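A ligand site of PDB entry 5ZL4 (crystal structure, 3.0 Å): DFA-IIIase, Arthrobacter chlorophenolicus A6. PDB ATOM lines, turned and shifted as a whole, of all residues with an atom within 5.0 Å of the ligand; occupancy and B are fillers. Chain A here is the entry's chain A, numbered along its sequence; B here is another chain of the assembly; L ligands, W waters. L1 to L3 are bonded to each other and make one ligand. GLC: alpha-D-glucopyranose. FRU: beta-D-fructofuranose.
Ser 84 touches the ligand.
CD1 of Ile 85 touches O3 of FRU L2 (3.6 Å).
CA of Gly 232 touches O4 of FRU L3, 3.99 Å away.
CE1 of Phe 256 touches O4 of FRU L3, at 3.8 Å.
Phe 281 touches the ligand.
Pro 308 touches the ligand.
CZ3 of Trp 309 touches O1 of FRU L3, at 3.3 Å.
Asp 177 of chain B touches the ligand.
CB of Asp 199 of chain B touches O4 of FRU L2, at 3.7 Å.
CG of Gln 222 of chain B touches C6 of GLC L1, 3.6 Å away.
CB of Ala 223 of chain B touches O6 of FRU L2 (3.7 Å).
Hydrophobic or aromatic side chains that line the ligand: Ile 85, Phe 256, Pro 257, Phe 281, Pro 308, Trp 309 and Ala 223 of chain B.
Of the 21 residues printed, 15 come within 4 Å of the ligand.
The nearest printed residue that does not touch the ligand is Ala 233 (4.3 Å).
An oxygen (O4) of FRU L3 lies within hydrogen-bond range of the backbone carbonyl oxygen (O) of Pro 257, 2.6 Å away.
The side-chain carboxylate of Glu 210 lies within hydrogen-bond range of an oxygen (O3) of FRU L3, 2.7 Å away.
NH1 of Arg 134 of chain B sits at hydrogen-bond distance from O4 of FRU L2 (3.1 Å).
NH1 of Arg 258 lies within hydrogen-bond range of O5 of FRU L3, at 3.2 Å.
O of Gly 232 lies within hydrogen-bond range of N of Glu 210, 3.2 Å away.
The side-chain carboxylate (OE2) of Glu 210 lies within hydrogen-bond range of the side-chain hydroxyl (OG) of Ser 82 (2.7 Å).
OD2 of Asp 177 of chain B lies within salt-bridge range of NH2 of Arg 134 of chain B (3.3 Å).
OD2 of Asp 199 of chain B is in salt-bridge range of NH1 of Arg 134 of chain B (2.9 Å).
The guanidinium group (NE) of Arg 258 lies within salt-bridge range of the side-chain carboxylate (OE1) of Glu 307 (2.9 Å).
N of Trp 309 lies close to OE2 of Glu 307.
OD1 of Asp 199 of chain B lies close to N of Gln 222 of chain B (3.4 Å).
N of Ile 85 lies within hydrogen-bond range of OG of Ser 82 (3.1 Å).
Water W1 lies within hydrogen-bond range of an oxygen (O4) of FRU L3 (2.7 Å), the backbone carbonyl oxygen (O) of Ala 233 (2.7 Å), the side-chain hydroxyl (OH) of Tyr 163 (2.8 Å), the backbone NH (N) of Glu 210 (3.2 Å) and the backbone carbonyl oxygen (O) of Gly 232 (3.4 Å).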
ATOM      1  N   PHE A  80      27.939  23.408  31.216  1.00  0.00           N
ATOM      2  CA  PHE A  80      28.342  23.041  29.857  1.00  0.00           C
ATOM      3  C   PHE A  80      27.981  24.150  28.855  1.00  0.00           C
ATOM      4  O   PHE A  80      26.846  24.606  28.808  1.00  0.00           O
ATOM      5  CB  PHE A  80      27.686  21.730  29.411  1.00  0.00           C
ATOM      6  CG  PHE A  80      28.039  21.327  28.000  1.00  0.00           C
ATOM      7  CD1 PHE A  80      27.280  21.781  26.929  1.00  0.00           C
ATOM      8  CD2 PHE A  80      29.139  20.522  27.746  1.00  0.00           C
ATOM      9  CE1 PHE A  80      27.601  21.430  25.625  1.00  0.00           C
ATOM     10  CE2 PHE A  80      29.471  20.175  26.449  1.00  0.00           C
ATOM     11  CZ  PHE A  80      28.704  20.628  25.393  1.00  0.00           C
ATOM     12  N   SER A  82      29.264  24.567  24.511  1.00  0.00           N
ATOM     13  CA  SER A  82      29.970  23.801  23.459  1.00  0.00           C
ATOM     14  C   SER A  82      31.300  24.435  23.036  1.00  0.00           C
ATOM     15  O   SER A  82      31.328  25.235  22.093  1.00  0.00           O
ATOM     16  CB  SER A  82      29.073  23.597  22.236  1.00  0.00           C
ATOM     17  OG  SER A  82      29.809  23.043  21.150  1.00  0.00           O
ATOM     18  N   SER A  84      33.591  22.923  21.461  1.00  0.00           N
ATOM     19  CA  SER A  84      33.792  22.483  20.082  1.00  0.00           C
ATOM     20  C   SER A  84      33.277  23.503  19.079  1.00  0.00           C
ATOM     21  O   SER A  84      34.000  23.882  18.166  1.00  0.00           O
ATOM     22  CB  SER A  84      33.112  21.140  19.845  1.00  0.00           C
ATOM     23  OG  SER A  84      33.285  20.711  18.504  1.00  0.00           O
ATOM     24  N   ILE A  85      32.043  23.968  19.263  1.00  0.00           N
ATOM     25  CA  ILE A  85      31.475  24.970  18.361  1.00  0.00           C
ATOM     26  C   ILE A  85      32.328  26.234  18.348  1.00  0.00           C
ATOM     27  O   ILE A  85      32.731  26.685  17.279  1.00  0.00           O
ATOM     28  CB  ILE A  85      29.981  25.271  18.669  1.00  0.00           C
ATOM     29  CG1 ILE A  85      29.118  24.180  18.011  1.00  0.00           C
ATOM     30  CG2 ILE A  85      29.558  26.647  18.144  1.00  0.00           C
ATOM     31  CD1 ILE A  85      27.702  24.073  18.539  1.00  0.00           C
ATOM     32  N   TYR A 163      40.109  15.463  19.887  1.00  0.00           N
ATOM     33  CA  TYR A 163      39.617  14.770  21.080  1.00  0.00           C
ATOM     34  C   TYR A 163      40.773  14.121  21.868  1.00  0.00           C
ATOM     35  O   TYR A 163      40.638  13.015  22.396  1.00  0.00           O
ATOM     36  CB  TYR A 163      38.532  13.739  20.737  1.00  0.00           C
ATOM     37  CG  TYR A 163      37.182  14.289  20.328  1.00  0.00           C
ATOM     38  CD1 TYR A 163      36.208  14.583  21.289  1.00  0.00           C
ATOM     39  CD2 TYR A 163      36.829  14.452  18.981  1.00  0.00           C
ATOM     40  CE1 TYR A 163      34.950  15.049  20.929  1.00  0.00           C
ATOM     41  CE2 TYR A 163      35.572  14.913  18.609  1.00  0.00           C
ATOM     42  CZ  TYR A 163      34.634  15.216  19.577  1.00  0.00           C
ATOM     43  OH  TYR A 163      33.379  15.679  19.226  1.00  0.00           O
ATOM     44  N   ALA A 209      29.620  15.448  27.340  1.00  0.00           N
ATOM     45  CA  ALA A 209      29.730  15.750  25.913  1.00  0.00           C
ATOM     46  C   ALA A 209      31.072  16.353  25.534  1.00  0.00           C
ATOM     47  O   ALA A 209      31.755  16.929  26.377  1.00  0.00           O
ATOM     48  CB  ALA A 209      28.613  16.672  25.487  1.00  0.00           C
ATOM     49  N   GLU A 210      31.399  16.222  24.243  1.00  0.00           N
ATOM     50  CA  GLU A 210      32.650  16.731  23.671  1.00  0.00           C
ATOM     51  C   GLU A 210      33.865  16.242  24.455  1.00  0.00           C
ATOM     52  O   GLU A 210      34.776  17.012  24.801  1.00  0.00           O
ATOM     53  CB  GLU A 210      32.583  18.253  23.518  1.00  0.00           C
ATOM     54  CG  GLU A 210      31.563  18.683  22.478  1.00  0.00           C
ATOM     55  CD  GLU A 210      31.209  20.154  22.532  1.00  0.00           C
ATOM     56  OE1 GLU A 210      32.021  20.939  23.078  1.00  0.00           O
ATOM     57  OE2 GLU A 210      30.120  20.526  22.012  1.00  0.00           O
ATOM     58  N   GLY A 232      27.744  12.422  24.381  1.00  0.00           N
ATOM     59  CA  GLY A 232      28.332  12.632  23.065  1.00  0.00           C
ATOM     60  C   GLY A 232      29.835  12.504  23.177  1.00  0.00           C
ATOM     61  O   GLY A 232      30.461  13.178  23.992  1.00  0.00           O
ATOM     62  N   ALA A 233      30.421  11.634  22.353  1.00  0.00           N
ATOM     63  CA  ALA A 233      31.855  11.371  22.413  1.00  0.00           C
ATOM     64  C   ALA A 233      32.561  11.754  21.100  1.00  0.00           C
ATOM     65  O   ALA A 233      31.970  12.454  20.254  1.00  0.00           O
ATOM     66  CB  ALA A 233      32.077   9.905  22.764  1.00  0.00           C
ATOM     67  N   PHE A 256      24.029  11.026  21.590  1.00  0.00           N
ATOM     68  CA  PHE A 256      24.197  11.689  20.286  1.00  0.00           C
ATOM     69  C   PHE A 256      25.637  11.464  19.783  1.00  0.00           C
ATOM     70  O   PHE A 256      26.451  10.861  20.498  1.00  0.00           O
ATOM     71  CB  PHE A 256      23.788  13.194  20.352  1.00  0.00           C
ATOM     72  CG  PHE A 256      24.291  13.948  21.551  1.00  0.00           C
ATOM     73  CD1 PHE A 256      25.507  14.608  21.519  1.00  0.00           C
ATOM     74  CD2 PHE A 256      23.535  14.037  22.712  1.00  0.00           C
ATOM     75  CE1 PHE A 256      25.969  15.328  22.606  1.00  0.00           C
ATOM     76  CE2 PHE A 256      23.987  14.742  23.811  1.00  0.00           C
ATOM     77  CZ  PHE A 256      25.202  15.383  23.764  1.00  0.00           C
ATOM     78  N   PRO A 257      25.950  11.884  18.534  1.00  0.00           N
ATOM     79  CA  PRO A 257      27.313  11.696  18.032  1.00  0.00           C
ATOM     80  C   PRO A 257      28.380  12.453  18.855  1.00  0.00           C
ATOM     81  O   PRO A 257      28.020  13.289  19.676  1.00  0.00           O
ATOM     82  CB  PRO A 257      27.219  12.241  16.590  1.00  0.00           C
ATOM     83  CG  PRO A 257      25.793  12.035  16.227  1.00  0.00           C
ATOM     84  CD  PRO A 257      25.038  12.341  17.471  1.00  0.00           C
ATOM     85  N   ARG A 258      29.673  12.202  18.646  1.00  0.00           N
ATOM     86  CA  ARG A 258      30.220  11.428  17.544  1.00  0.00           C
ATOM     87  C   ARG A 258      31.215  10.386  18.036  1.00  0.00           C
ATOM     88  O   ARG A 258      32.332  10.299  17.541  1.00  0.00           O
ATOM     89  CB  ARG A 258      30.860  12.365  16.504  1.00  0.00           C
ATOM     90  CG  ARG A 258      31.890  13.348  17.045  1.00  0.00           C
ATOM     91  CD  ARG A 258      32.476  14.184  15.918  1.00  0.00           C
ATOM     92  NE  ARG A 258      31.447  14.990  15.263  1.00  0.00           N
ATOM     93  CZ  ARG A 258      30.997  16.179  15.686  1.00  0.00           C
ATOM     94  NH1 ARG A 258      31.493  16.747  16.789  1.00  0.00           N
ATOM     95  NH2 ARG A 258      30.040  16.794  14.998  1.00  0.00           N
ATOM     96  N   PHE A 281      26.876   9.038  13.583  1.00  0.00           N
ATOM     97  CA  PHE A 281      27.167   9.319  12.189  1.00  0.00           C
ATOM     98  C   PHE A 281      27.922   8.174  11.503  1.00  0.00           C
ATOM     99  O   PHE A 281      28.232   8.273  10.319  1.00  0.00           O
ATOM    100  CB  PHE A 281      27.969  10.632  12.053  1.00  0.00           C
ATOM    101  CG  PHE A 281      27.232  11.871  12.514  1.00  0.00           C
ATOM    102  CD1 PHE A 281      25.902  12.104  12.170  1.00  0.00           C
ATOM    103  CD2 PHE A 281      27.909  12.856  13.250  1.00  0.00           C
ATOM    104  CE1 PHE A 281      25.251  13.263  12.571  1.00  0.00           C
ATOM    105  CE2 PHE A 281      27.256  14.020  13.664  1.00  0.00           C
ATOM    106  CZ  PHE A 281      25.927  14.224  13.324  1.00  0.00           C
ATOM    107  N   GLU A 307      27.191  12.803   8.966  1.00  0.00           N
ATOM    108  CA  GLU A 307      27.624  14.056   9.621  1.00  0.00           C
ATOM    109  C   GLU A 307      27.296  15.270   8.741  1.00  0.00           C
ATOM    110  O   GLU A 307      27.732  15.304   7.594  1.00  0.00           O
ATOM    111  CB  GLU A 307      29.137  13.999   9.859  1.00  0.00           C
ATOM    112  CG  GLU A 307      29.782  15.305  10.298  1.00  0.00           C
ATOM    113  CD  GLU A 307      29.691  15.525  11.789  1.00  0.00           C
ATOM    114  OE1 GLU A 307      30.466  14.861  12.510  1.00  0.00           O
ATOM    115  OE2 GLU A 307      28.870  16.372  12.235  1.00  0.00           O
ATOM    116  N   PRO A 308      26.561  16.273   9.271  1.00  0.00           N
ATOM    117  CA  PRO A 308      26.260  17.489   8.493  1.00  0.00           C
ATOM    118  C   PRO A 308      27.195  18.674   8.763  1.00  0.00           C
ATOM    119  O   PRO A 308      27.228  19.615   7.963  1.00  0.00           O
ATOM    120  CB  PRO A 308      24.857  17.841   8.950  1.00  0.00           C
ATOM    121  CG  PRO A 308      24.850  17.446  10.384  1.00  0.00           C
ATOM    122  CD  PRO A 308      25.772  16.258  10.515  1.00  0.00           C
ATOM    123  N   TRP A 309      27.917  18.633   9.889  1.00  0.00           N
ATOM    124  CA  TRP A 309      28.736  19.748  10.313  1.00  0.00           C
ATOM    125  C   TRP A 309      30.078  19.710   9.583  1.00  0.00           C
ATOM    126  O   TRP A 309      30.849  18.767   9.742  1.00  0.00           O
ATOM    127  CB  TRP A 309      28.944  19.703  11.837  1.00  0.00           C
ATOM    128  CG  TRP A 309      29.425  20.999  12.410  1.00  0.00           C
ATOM    129  CD1 TRP A 309      29.078  22.256  12.015  1.00  0.00           C
ATOM    130  CD2 TRP A 309      30.343  21.172  13.501  1.00  0.00           C
ATOM    131  NE1 TRP A 309      29.726  23.190  12.776  1.00  0.00           N
ATOM    132  CE2 TRP A 309      30.499  22.558  13.697  1.00  0.00           C
ATOM    133  CE3 TRP A 309      31.038  20.282  14.333  1.00  0.00           C
ATOM    134  CZ2 TRP A 309      31.336  23.089  14.694  1.00  0.00           C
ATOM    135  CZ3 TRP A 309      31.865  20.804  15.311  1.00  0.00           C
ATOM    136  CH2 TRP A 309      32.008  22.195  15.480  1.00  0.00           C
ATOM    137  N   ARG B 134      24.465  29.957  21.835  1.00  0.00           N
ATOM    138  CA  ARG B 134      23.193  29.674  22.492  1.00  0.00           C
ATOM    139  C   ARG B 134      23.349  29.831  24.007  1.00  0.00           C
ATOM    140  O   ARG B 134      24.367  29.431  24.578  1.00  0.00           O
ATOM    141  CB  ARG B 134      22.705  28.264  22.168  1.00  0.00           C
ATOM    142  CG  ARG B 134      22.358  28.027  20.705  1.00  0.00           C
ATOM    143  CD  ARG B 134      22.298  26.540  20.405  1.00  0.00           C
ATOM    144  NE  ARG B 134      23.629  25.912  20.477  1.00  0.00           N
ATOM    145  CZ  ARG B 134      23.865  24.596  20.526  1.00  0.00           C
ATOM    146  NH1 ARG B 134      22.863  23.713  20.528  1.00  0.00           N
ATOM    147  NH2 ARG B 134      25.123  24.151  20.596  1.00  0.00           N
ATOM    148  N   ASP B 177      20.964  25.518  24.897  1.00  0.00           N
ATOM    149  CA  ASP B 177      21.723  24.262  24.865  1.00  0.00           C
ATOM    150  C   ASP B 177      21.949  23.816  26.311  1.00  0.00           C
ATOM    151  O   ASP B 177      22.308  24.634  27.152  1.00  0.00           O
ATOM    152  CB  ASP B 177      23.076  24.468  24.140  1.00  0.00           C
ATOM    153  CG  ASP B 177      23.851  23.156  23.871  1.00  0.00           C
ATOM    154  OD1 ASP B 177      23.254  22.056  23.752  1.00  0.00           O
ATOM    155  OD2 ASP B 177      25.094  23.246  23.730  1.00  0.00           O
ATOM    156  N   ASP B 199      17.960  22.655  22.503  1.00  0.00           N
ATOM    157  CA  ASP B 199      18.931  21.600  22.198  1.00  0.00           C
ATOM    158  C   ASP B 199      19.441  20.971  23.497  1.00  0.00           C
ATOM    159  O   ASP B 199      19.775  21.680  24.439  1.00  0.00           O
ATOM    160  CB  ASP B 199      20.098  22.175  21.386  1.00  0.00           C
ATOM    161  CG  ASP B 199      19.675  22.622  19.991  1.00  0.00           C
ATOM    162  OD1 ASP B 199      18.919  21.869  19.347  1.00  0.00           O
ATOM    163  OD2 ASP B 199      20.103  23.703  19.530  1.00  0.00           O
ATOM    164  N   GLN B 222      16.402  19.592  19.359  1.00  0.00           N
ATOM    165  CA  GLN B 222      17.185  18.393  19.101  1.00  0.00           C
ATOM    166  C   GLN B 222      17.703  17.747  20.370  1.00  0.00           C
ATOM    167  O   GLN B 222      18.078  18.433  21.332  1.00  0.00           O
ATOM    168  CB  GLN B 222      18.397  18.740  18.238  1.00  0.00           C
ATOM    169  CG  GLN B 222      18.063  19.092  16.789  1.00  0.00           C
ATOM    170  CD  GLN B 222      17.522  17.938  15.971  1.00  0.00           C
ATOM    171  OE1 GLN B 222      16.764  18.156  15.016  1.00  0.00           O
ATOM    172  NE2 GLN B 222      17.894  16.685  16.321  1.00  0.00           N
ATOM    173  N   ALA B 223      17.734  16.409  20.355  1.00  0.00           N
ATOM    174  CA  ALA B 223      18.441  15.594  21.335  1.00  0.00           C
ATOM    175  C   ALA B 223      18.061  15.891  22.792  1.00  0.00           C
ATOM    176  O   ALA B 223      18.906  15.841  23.674  1.00  0.00           O
ATOM    177  CB  ALA B 223      19.946  15.744  21.125  1.00  0.00           C
HETATM  178  C1  GLC L   1      24.437  18.838  15.411  1.00  0.00           C
HETATM  179  C2  GLC L   1      25.018  19.213  14.067  1.00  0.00           C
HETATM  180  C3  GLC L   1      24.303  20.399  13.460  1.00  0.00           C
HETATM  181  C4  GLC L   1      22.812  20.160  13.416  1.00  0.00           C
HETATM  182  C5  GLC L   1      22.306  19.690  14.758  1.00  0.00           C
HETATM  183  C6  GLC L   1      20.898  19.160  14.585  1.00  0.00           C
HETATM  184  O2  GLC L   1      26.372  19.576  14.241  1.00  0.00           O
HETATM  185  O3  GLC L   1      24.781  20.618  12.131  1.00  0.00           O
HETATM  186  O4  GLC L   1      22.167  21.366  13.029  1.00  0.00           O
HETATM  187  O5  GLC L   1      23.058  18.616  15.271  1.00  0.00           O
HETATM  188  O6  GLC L   1      20.950  17.944  13.838  1.00  0.00           O
HETATM  189  C1  FRU L   2      26.700  19.306  17.426  1.00  0.00           C
HETATM  190  C2  FRU L   2      25.200  19.520  17.569  1.00  0.00           C
HETATM  191  C3  FRU L   2      24.903  20.583  18.581  1.00  0.00           C
HETATM  192  C4  FRU L   2      23.558  20.169  19.084  1.00  0.00           C
HETATM  193  C5  FRU L   2      23.667  18.666  19.096  1.00  0.00           C
HETATM  194  C6  FRU L   2      22.302  17.999  18.972  1.00  0.00           C
HETATM  195  O1  FRU L   2      27.328  19.186  18.705  1.00  0.00           O
HETATM  196  O2  FRU L   2      24.625  19.894  16.333  1.00  0.00           O
HETATM  197  O3  FRU L   2      24.854  21.891  18.019  1.00  0.00           O
HETATM  198  O4  FRU L   2      23.314  20.678  20.387  1.00  0.00           O
HETATM  199  O5  FRU L   2      24.534  18.357  18.002  1.00  0.00           O
HETATM  200  O6  FRU L   2      22.444  16.657  18.483  1.00  0.00           O
HETATM  201  C1  FRU L   3      29.705  19.489  18.332  1.00  0.00           C
HETATM  202  C2  FRU L   3      28.603  18.541  18.663  1.00  0.00           C
HETATM  203  C3  FRU L   3      28.915  17.904  19.978  1.00  0.00           C
HETATM  204  C4  FRU L   3      28.254  16.574  19.859  1.00  0.00           C
HETATM  205  C5  FRU L   3      28.149  16.311  18.374  1.00  0.00           C
HETATM  206  C6  FRU L   3      26.740  16.065  17.891  1.00  0.00           C
HETATM  207  O1  FRU L   3      29.254  20.144  17.180  1.00  0.00           O
HETATM  208  O3  FRU L   3      28.436  18.699  21.040  1.00  0.00           O
HETATM  209  O4  FRU L   3      29.056  15.579  20.468  1.00  0.00           O
HETATM  210  O5  FRU L   3      28.569  17.482  17.733  1.00  0.00           O
HETATM  211  O6  FRU L   3      26.799  15.921  16.490  1.00  0.00           O
HETATM  212  O   HOH W   1      31.557  14.964  21.290  1.00  0.00           O
HETATM  213  O   HOH W   2      21.355  14.480  18.038  1.00  0.00           O
HETATM  214  O   HOH W   3      25.633  19.747  22.429  1.00  0.00           O
